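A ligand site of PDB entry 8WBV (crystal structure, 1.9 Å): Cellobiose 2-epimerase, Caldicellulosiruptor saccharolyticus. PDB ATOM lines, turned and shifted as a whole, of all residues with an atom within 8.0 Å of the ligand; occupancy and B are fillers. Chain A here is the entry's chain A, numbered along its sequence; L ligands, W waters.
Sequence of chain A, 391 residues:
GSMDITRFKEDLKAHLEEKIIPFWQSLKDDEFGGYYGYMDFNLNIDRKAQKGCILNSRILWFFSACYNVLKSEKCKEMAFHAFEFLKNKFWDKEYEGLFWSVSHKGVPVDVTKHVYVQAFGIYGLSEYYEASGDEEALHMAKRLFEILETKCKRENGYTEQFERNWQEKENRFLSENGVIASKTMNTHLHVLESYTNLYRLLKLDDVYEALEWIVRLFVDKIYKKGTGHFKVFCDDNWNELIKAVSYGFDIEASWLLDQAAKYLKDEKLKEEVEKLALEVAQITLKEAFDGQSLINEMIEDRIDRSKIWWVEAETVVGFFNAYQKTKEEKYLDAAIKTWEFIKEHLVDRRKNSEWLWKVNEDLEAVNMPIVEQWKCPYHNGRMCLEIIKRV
An oxygen (O3) of the ligand sits at hydrogen-bond distance from the side-chain carboxylate of Glu 168.
The side-chain amino group of Lys 183 sits at hydrogen-bond distance from an oxygen (O1) of the ligand (3.4 Å).
An oxygen (O6) of the ligand lies within hydrogen-bond range of the side-chain hydroxyl (OG) of Ser 182 (2.7 Å).
O of Lys 169 sits at hydrogen-bond distance from O2 of the ligand (2.9 Å).
An oxygen (O1) of the ligand is in hydrogen-bond range of the side-chain carboxylate of Asp 236, 2.6 Å away.
The side-chain amino group of Lys 183 sits at hydrogen-bond distance from the backbone carbonyl oxygen of Tyr 158 (3.1 Å).
The backbone carbonyl oxygen (O) of Cys 234 is in hydrogen-bond range of the backbone NH (N) of Ser 182.
O of Lys 183 lies within hydrogen-bond range of N of Cys 234 (2.8 Å).
OD1 of Asp 236 is in salt-bridge range of NZ of Lys 183, 2.8 Å away.
O of Asp 236 is in hydrogen-bond range of ND2 of Asn 156, at 2.8 Å.
OE1 of Glu 168 lies within salt-bridge range of NH2 of Arg 154 (3.0 Å).
N of Lys 169 lies within hydrogen-bond range of O of Gln 161 (3.0 Å).
The backbone NH (N) of Thr 159 is in hydrogen-bond range of the backbone carbonyl oxygen (O) of Cys 152 (3.1 Å).
CG2 of Thr 159 touches O2 of the ligand (3.8 Å).
CA of Glu 170 touches O2 of the ligand, 3.7 Å away.
The nearest printed residue that does not touch the ligand is Asn 171 (4.3 Å).
Water W3 lies within hydrogen-bond range of the backbone carbonyl oxygen of Ser 182 (2.6 Å), an oxygen (O1) of the ligand (2.8 Å) and the backbone NH of Glu 160 (3.1 Å).
Water W1 lies within hydrogen-bond range of O2 of the ligand (2.9 Å), N of Asn 171 (2.9 Å) and OG of Ser 182 (2.9 Å).
Water W2 lies within hydrogen-bond range of the backbone carbonyl oxygen of Lys 169 (2.8 Å), the backbone NH of Gln 161 (3.0 Å), an oxygen (O2) of the ligand (3.1 Å) and the backbone NH of Asn 171 (3.2 Å).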
ATOM      1  N   CYS A 152       4.385  30.783 -22.689  1.00  0.00           N
ATOM      2  CA  CYS A 152       3.043  30.276 -22.422  1.00  0.00           C
ATOM      3  C   CYS A 152       1.946  31.328 -22.393  1.00  0.00           C
ATOM      4  O   CYS A 152       0.783  30.993 -22.622  1.00  0.00           O
ATOM      5  CB  CYS A 152       3.014  29.514 -21.086  1.00  0.00           C
ATOM      6  SG  CYS A 152       4.311  28.206 -20.976  1.00  0.00           S
ATOM      7  N   ARG A 154      -0.603  34.343 -23.301  1.00  0.00           N
ATOM      8  CA  ARG A 154      -1.321  34.835 -24.474  1.00  0.00           C
ATOM      9  C   ARG A 154      -2.144  36.052 -24.071  1.00  0.00           C
ATOM     10  O   ARG A 154      -2.147  36.456 -22.909  1.00  0.00           O
ATOM     11  CB  ARG A 154      -2.214  33.742 -25.067  1.00  0.00           C
ATOM     12  CG  ARG A 154      -1.446  32.489 -25.472  1.00  0.00           C
ATOM     13  CD  ARG A 154      -0.541  32.721 -26.670  1.00  0.00           C
ATOM     14  NE  ARG A 154       0.036  31.475 -27.137  1.00  0.00           N
ATOM     15  CZ  ARG A 154       1.213  31.006 -26.739  1.00  0.00           C
ATOM     16  NH1 ARG A 154       1.929  31.713 -25.876  1.00  0.00           N
ATOM     17  NH2 ARG A 154       1.669  29.856 -27.193  1.00  0.00           N
ATOM     18  N   ASN A 156      -5.243  36.655 -23.516  1.00  0.00           N
ATOM     19  CA  ASN A 156      -6.299  36.535 -22.518  1.00  0.00           C
ATOM     20  C   ASN A 156      -6.001  35.462 -21.472  1.00  0.00           C
ATOM     21  O   ASN A 156      -6.932  34.892 -20.897  1.00  0.00           O
ATOM     22  CB  ASN A 156      -7.638  36.263 -23.188  1.00  0.00           C
ATOM     23  CG  ASN A 156      -7.621  35.000 -24.031  1.00  0.00           C
ATOM     24  OD1 ASN A 156      -6.597  34.307 -24.122  1.00  0.00           O
ATOM     25  ND2 ASN A 156      -8.752  34.695 -24.643  1.00  0.00           N
ATOM     26  N   GLY A 157      -4.723  35.187 -21.197  1.00  0.00           N
ATOM     27  CA  GLY A 157      -4.346  34.221 -20.182  1.00  0.00           C
ATOM     28  C   GLY A 157      -3.287  33.281 -20.701  1.00  0.00           C
ATOM     29  O   GLY A 157      -2.602  33.568 -21.693  1.00  0.00           O
ATOM     30  N   TYR A 158      -3.135  32.128 -20.058  1.00  0.00           N
ATOM     31  CA  TYR A 158      -2.079  31.185 -20.419  1.00  0.00           C
ATOM     32  C   TYR A 158      -2.647  30.046 -21.250  1.00  0.00           C
ATOM     33  O   TYR A 158      -3.680  29.467 -20.900  1.00  0.00           O
ATOM     34  CB  TYR A 158      -1.366  30.647 -19.175  1.00  0.00           C
ATOM     35  CG  TYR A 158      -0.653  31.739 -18.426  1.00  0.00           C
ATOM     36  CD1 TYR A 158      -1.318  32.500 -17.478  1.00  0.00           C
ATOM     37  CD2 TYR A 158       0.686  32.040 -18.690  1.00  0.00           C
ATOM     38  CE1 TYR A 158      -0.674  33.532 -16.798  1.00  0.00           C
ATOM     39  CE2 TYR A 158       1.337  33.053 -18.001  1.00  0.00           C
ATOM     40  CZ  TYR A 158       0.648  33.801 -17.071  1.00  0.00           C
ATOM     41  OH  TYR A 158       1.288  34.828 -16.398  1.00  0.00           O
ATOM     42  N   THR A 159      -1.992  29.739 -22.366  1.00  0.00           N
ATOM     43  CA  THR A 159      -2.137  28.416 -22.934  1.00  0.00           C
ATOM     44  C   THR A 159      -1.556  27.431 -21.919  1.00  0.00           C
ATOM     45  O   THR A 159      -0.492  27.680 -21.353  1.00  0.00           O
ATOM     46  CB  THR A 159      -1.414  28.335 -24.279  1.00  0.00           C
ATOM     47  OG1 THR A 159      -2.050  29.230 -25.208  1.00  0.00           O
ATOM     48  CG2 THR A 159      -1.444  26.912 -24.854  1.00  0.00           C
ATOM     49  N   GLU A 160      -2.286  26.353 -21.637  1.00  0.00           N
ATOM     50  CA  GLU A 160      -2.059  25.586 -20.415  1.00  0.00           C
ATOM     51  C   GLU A 160      -1.199  24.346 -20.603  1.00  0.00           C
ATOM     52  O   GLU A 160      -0.531  23.934 -19.649  1.00  0.00           O
ATOM     53  CB  GLU A 160      -3.416  25.195 -19.801  1.00  0.00           C
ATOM     54  CG  GLU A 160      -4.208  26.465 -19.408  1.00  0.00           C
ATOM     55  CD  GLU A 160      -5.384  26.200 -18.464  1.00  0.00           C
ATOM     56  OE1 GLU A 160      -5.559  25.054 -18.021  1.00  0.00           O
ATOM     57  OE2 GLU A 160      -6.134  27.162 -18.180  1.00  0.00           O
ATOM     58  N   GLN A 161      -1.154  23.768 -21.805  1.00  0.00           N
ATOM     59  CA  GLN A 161      -0.518  22.481 -22.031  1.00  0.00           C
ATOM     60  C   GLN A 161       0.435  22.567 -23.225  1.00  0.00           C
ATOM     61  O   GLN A 161       0.074  23.134 -24.266  1.00  0.00           O
ATOM     62  CB  GLN A 161      -1.549  21.387 -22.296  1.00  0.00           C
ATOM     63  CG  GLN A 161      -0.947  20.089 -22.794  1.00  0.00           C
ATOM     64  CD  GLN A 161      -0.390  19.254 -21.657  1.00  0.00           C
ATOM     65  OE1 GLN A 161      -1.131  18.549 -20.975  1.00  0.00           O
ATOM     66  NE2 GLN A 161       0.916  19.335 -21.441  1.00  0.00           N
ATOM     67  N   PHE A 162       1.621  21.983 -23.069  1.00  0.00           N
ATOM     68  CA  PHE A 162       2.673  22.057 -24.073  1.00  0.00           C
ATOM     69  C   PHE A 162       3.378  20.706 -24.164  1.00  0.00           C
ATOM     70  O   PHE A 162       3.459  19.969 -23.183  1.00  0.00           O
ATOM     71  CB  PHE A 162       3.703  23.137 -23.722  1.00  0.00           C
ATOM     72  CG  PHE A 162       3.101  24.519 -23.599  1.00  0.00           C
ATOM     73  CD1 PHE A 162       2.460  24.917 -22.432  1.00  0.00           C
ATOM     74  CD2 PHE A 162       3.167  25.404 -24.659  1.00  0.00           C
ATOM     75  CE1 PHE A 162       1.898  26.167 -22.336  1.00  0.00           C
ATOM     76  CE2 PHE A 162       2.605  26.666 -24.570  1.00  0.00           C
ATOM     77  CZ  PHE A 162       1.971  27.044 -23.394  1.00  0.00           C
ATOM     78  N   GLN A 167       6.263  23.362 -27.506  1.00  0.00           N
ATOM     79  CA  GLN A 167       5.279  23.606 -28.555  1.00  0.00           C
ATOM     80  C   GLN A 167       3.881  23.413 -27.995  1.00  0.00           C
ATOM     81  O   GLN A 167       3.627  22.468 -27.239  1.00  0.00           O
ATOM     82  CB  GLN A 167       5.517  22.675 -29.745  1.00  0.00           C
ATOM     83  CG  GLN A 167       6.857  22.900 -30.438  1.00  0.00           C
ATOM     84  CD  GLN A 167       7.094  21.933 -31.593  1.00  0.00           C
ATOM     85  OE1 GLN A 167       7.061  20.709 -31.404  1.00  0.00           O
ATOM     86  NE2 GLN A 167       7.345  22.473 -32.772  1.00  0.00           N
ATOM     87  N   GLU A 168       2.955  24.311 -28.328  1.00  0.00           N
ATOM     88  CA  GLU A 168       1.675  24.262 -27.636  1.00  0.00           C
ATOM     89  C   GLU A 168       0.832  23.073 -28.103  1.00  0.00           C
ATOM     90  O   GLU A 168       0.951  22.603 -29.230  1.00  0.00           O
ATOM     91  CB  GLU A 168       0.897  25.568 -27.814  1.00  0.00           C
ATOM     92  CG  GLU A 168       0.545  25.887 -29.230  1.00  0.00           C
ATOM     93  CD  GLU A 168      -0.190  27.218 -29.330  1.00  0.00           C
ATOM     94  OE1 GLU A 168       0.499  28.267 -29.417  1.00  0.00           O
ATOM     95  OE2 GLU A 168      -1.437  27.221 -29.293  1.00  0.00           O
ATOM     96  N   LYS A 169      -0.014  22.598 -27.192  1.00  0.00           N
ATOM     97  CA  LYS A 169      -0.961  21.521 -27.407  1.00  0.00           C
ATOM     98  C   LYS A 169      -2.335  22.010 -26.970  1.00  0.00           C
ATOM     99  O   LYS A 169      -2.459  23.015 -26.271  1.00  0.00           O
ATOM    100  CB  LYS A 169      -0.637  20.269 -26.583  1.00  0.00           C
ATOM    101  CG  LYS A 169       0.604  19.507 -26.958  1.00  0.00           C
ATOM    102  CD  LYS A 169       0.584  18.130 -26.305  1.00  0.00           C
ATOM    103  CE  LYS A 169      -0.538  17.268 -26.877  1.00  0.00           C
ATOM    104  NZ  LYS A 169      -0.624  15.940 -26.222  1.00  0.00           N
ATOM    105  N   GLU A 170      -3.361  21.278 -27.377  1.00  0.00           N
ATOM    106  CA  GLU A 170      -4.660  21.446 -26.749  1.00  0.00           C
ATOM    107  C   GLU A 170      -4.609  20.926 -25.310  1.00  0.00           C
ATOM    108  O   GLU A 170      -3.783  20.090 -24.953  1.00  0.00           O
ATOM    109  CB  GLU A 170      -5.745  20.716 -27.540  1.00  0.00           C
ATOM    110  CG  GLU A 170      -5.700  19.204 -27.375  1.00  0.00           C
ATOM    111  CD  GLU A 170      -4.830  18.532 -28.419  1.00  0.00           C
ATOM    112  OE1 GLU A 170      -3.988  19.216 -29.048  1.00  0.00           O
ATOM    113  OE2 GLU A 170      -5.006  17.316 -28.614  1.00  0.00           O
ATOM    114  N   ASN A 171      -5.527  21.417 -24.501  1.00  0.00           N
ATOM    115  CA  ASN A 171      -5.390  21.150 -23.073  1.00  0.00           C
ATOM    116  C   ASN A 171      -5.775  19.714 -22.726  1.00  0.00           C
ATOM    117  O   ASN A 171      -6.486  19.046 -23.475  1.00  0.00           O
ATOM    118  CB  ASN A 171      -6.263  22.117 -22.279  1.00  0.00           C
ATOM    119  CG  ASN A 171      -5.727  22.356 -20.886  1.00  0.00           C
ATOM    120  OD1 ASN A 171      -4.732  21.737 -20.481  1.00  0.00           O
ATOM    121  ND2 ASN A 171      -6.364  23.256 -20.143  1.00  0.00           N
ATOM    122  N   ARG A 172      -5.315  19.260 -21.562  1.00  0.00           N
ATOM    123  CA  ARG A 172      -5.655  17.935 -21.051  1.00  0.00           C
ATOM    124  C   ARG A 172      -6.854  17.935 -20.109  1.00  0.00           C
ATOM    125  O   ARG A 172      -7.397  16.859 -19.846  1.00  0.00           O
ATOM    126  CB  ARG A 172      -4.447  17.319 -20.331  1.00  0.00           C
ATOM    127  CG  ARG A 172      -4.095  17.982 -18.998  1.00  0.00           C
ATOM    128  CD  ARG A 172      -2.714  17.498 -18.501  1.00  0.00           C
ATOM    129  NE  ARG A 172      -2.774  16.099 -18.084  1.00  0.00           N
ATOM    130  CZ  ARG A 172      -1.786  15.220 -18.192  1.00  0.00           C
ATOM    131  NH1 ARG A 172      -0.615  15.554 -18.715  1.00  0.00           N
ATOM    132  NH2 ARG A 172      -1.983  13.984 -17.759  1.00  0.00           N
ATOM    133  N   ILE A 180     -12.791  19.714 -24.340  1.00  0.00           N
ATOM    134  CA  ILE A 180     -11.541  20.285 -23.842  1.00  0.00           C
ATOM    135  C   ILE A 180     -11.786  21.703 -23.342  1.00  0.00           C
ATOM    136  O   ILE A 180     -12.443  22.515 -24.015  1.00  0.00           O
ATOM    137  CB  ILE A 180     -10.459  20.260 -24.940  1.00  0.00           C
ATOM    138  CG1 ILE A 180     -10.043  18.814 -25.237  1.00  0.00           C
ATOM    139  CG2 ILE A 180      -9.244  21.087 -24.509  1.00  0.00           C
ATOM    140  CD1 ILE A 180      -9.258  18.648 -26.534  1.00  0.00           C
ATOM    141  N   ALA A 181     -11.284  22.000 -22.149  1.00  0.00           N
ATOM    142  CA  ALA A 181     -11.402  23.324 -21.526  1.00  0.00           C
ATOM    143  C   ALA A 181     -10.078  24.040 -21.750  1.00  0.00           C
ATOM    144  O   ALA A 181      -9.096  23.773 -21.059  1.00  0.00           O
ATOM    145  CB  ALA A 181     -11.748  23.199 -20.048  1.00  0.00           C
ATOM    146  N   SER A 182     -10.045  24.919 -22.750  1.00  0.00           N
ATOM    147  CA  SER A 182      -8.779  25.590 -23.083  1.00  0.00           C
ATOM    148  C   SER A 182      -8.358  26.604 -22.046  1.00  0.00           C
ATOM    149  O   SER A 182      -7.209  27.058 -22.079  1.00  0.00           O
ATOM    150  CB  SER A 182      -8.884  26.263 -24.462  1.00  0.00           C
ATOM    151  OG  SER A 182      -9.343  25.333 -25.443  1.00  0.00           O
ATOM    152  N   LYS A 183      -9.264  26.973 -21.139  1.00  0.00           N
ATOM    153  CA  LYS A 183      -8.992  27.929 -20.055  1.00  0.00           C
ATOM    154  C   LYS A 183      -9.624  27.384 -18.783  1.00  0.00           C
ATOM    155  O   LYS A 183     -10.838  27.144 -18.750  1.00  0.00           O
ATOM    156  CB  LYS A 183      -9.564  29.313 -20.386  1.00  0.00           C
ATOM    157  CG  LYS A 183      -8.791  30.008 -21.529  1.00  0.00           C
ATOM    158  CD  LYS A 183      -7.446  30.547 -21.006  1.00  0.00           C
ATOM    159  CE  LYS A 183      -6.556  30.994 -22.153  1.00  0.00           C
ATOM    160  NZ  LYS A 183      -6.027  29.816 -22.909  1.00  0.00           N
ATOM    161  N   CYS A 234     -13.583  26.593 -19.226  1.00  0.00           N
ATOM    162  CA  CYS A 234     -13.927  27.576 -20.243  1.00  0.00           C
ATOM    163  C   CYS A 234     -13.345  27.188 -21.593  1.00  0.00           C
ATOM    164  O   CYS A 234     -12.403  26.395 -21.682  1.00  0.00           O
ATOM    165  CB  CYS A 234     -13.414  28.947 -19.828  1.00  0.00           C
ATOM    166  SG  CYS A 234     -14.548  29.642 -18.600  1.00  0.00           S
ATOM    167  N   ASP A 235     -13.880  27.798 -22.650  1.00  0.00           N
ATOM    168  CA  ASP A 235     -13.241  27.716 -23.953  1.00  0.00           C
ATOM    169  C   ASP A 235     -12.020  28.639 -23.946  1.00  0.00           C
ATOM    170  O   ASP A 235     -11.618  29.172 -22.904  1.00  0.00           O
ATOM    171  CB  ASP A 235     -14.228  28.069 -25.068  1.00  0.00           C
ATOM    172  CG  ASP A 235     -14.732  29.531 -24.995  1.00  0.00           C
ATOM    173  OD1 ASP A 235     -14.123  30.346 -24.288  1.00  0.00           O
ATOM    174  OD2 ASP A 235     -15.737  29.833 -25.683  1.00  0.00           O
ATOM    175  N   ASP A 236     -11.428  28.877 -25.119  1.00  0.00           N
ATOM    176  CA  ASP A 236     -10.238  29.719 -25.174  1.00  0.00           C
ATOM    177  C   ASP A 236     -10.539  31.201 -24.958  1.00  0.00           C
ATOM    178  O   ASP A 236      -9.616  32.015 -24.951  1.00  0.00           O
ATOM    179  CB  ASP A 236      -9.516  29.543 -26.510  1.00  0.00           C
ATOM    180  CG  ASP A 236      -8.003  29.724 -26.412  1.00  0.00           C
ATOM    181  OD1 ASP A 236      -7.424  29.412 -25.359  1.00  0.00           O
ATOM    182  OD2 ASP A 236      -7.386  30.166 -27.405  1.00  0.00           O
ATOM    183  N   ASN A 237     -11.809  31.572 -24.795  1.00  0.00           N
ATOM    184  CA  ASN A 237     -12.203  32.969 -24.659  1.00  0.00           C
ATOM    185  C   ASN A 237     -12.901  33.222 -23.319  1.00  0.00           C
ATOM    186  O   ASN A 237     -13.676  34.174 -23.197  1.00  0.00           O
ATOM    187  CB  ASN A 237     -13.110  33.371 -25.834  1.00  0.00           C
ATOM    188  CG  ASN A 237     -12.342  33.486 -27.146  1.00  0.00           C
ATOM    189  OD1 ASN A 237     -11.809  34.542 -27.468  1.00  0.00           O
ATOM    190  ND2 ASN A 237     -12.291  32.403 -27.914  1.00  0.00           N
HETATM  191  C1  LIG L   1      -5.562  27.215 -26.801  1.00  0.00           C
HETATM  192  C2  LIG L   1      -4.376  26.346 -27.184  1.00  0.00           C
HETATM  193  C3  LIG L   1      -4.451  25.962 -28.604  1.00  0.00           C
HETATM  194  C4  LIG L   1      -5.749  25.281 -28.943  1.00  0.00           C
HETATM  195  C5  LIG L   1      -6.968  26.072 -28.442  1.00  0.00           C
HETATM  196  C6  LIG L   1      -8.211  25.258 -28.648  1.00  0.00           C
HETATM  197  O1  LIG L   1      -5.472  27.633 -25.501  1.00  0.00           O
HETATM  198  O2  LIG L   1      -4.412  25.141 -26.401  1.00  0.00           O
HETATM  199  O3  LIG L   1      -3.338  25.072 -28.884  1.00  0.00           O
HETATM  200  O4  LIG L   1      -5.863  25.136 -30.352  1.00  0.00           O
HETATM  201  O5  LIG L   1      -6.826  26.423 -27.011  1.00  0.00           O
HETATM  202  O6  LIG L   1      -9.300  25.950 -28.073  1.00  0.00           O
HETATM  203  O   HOH W   1      -6.787  23.867 -25.458  1.00  0.00           O
HETATM  204  O   HOH W   2      -3.455  23.700 -23.792  1.00  0.00           O
HETATM  205  O   HOH W   3      -4.991  26.226 -23.176  1.00  0.00           O
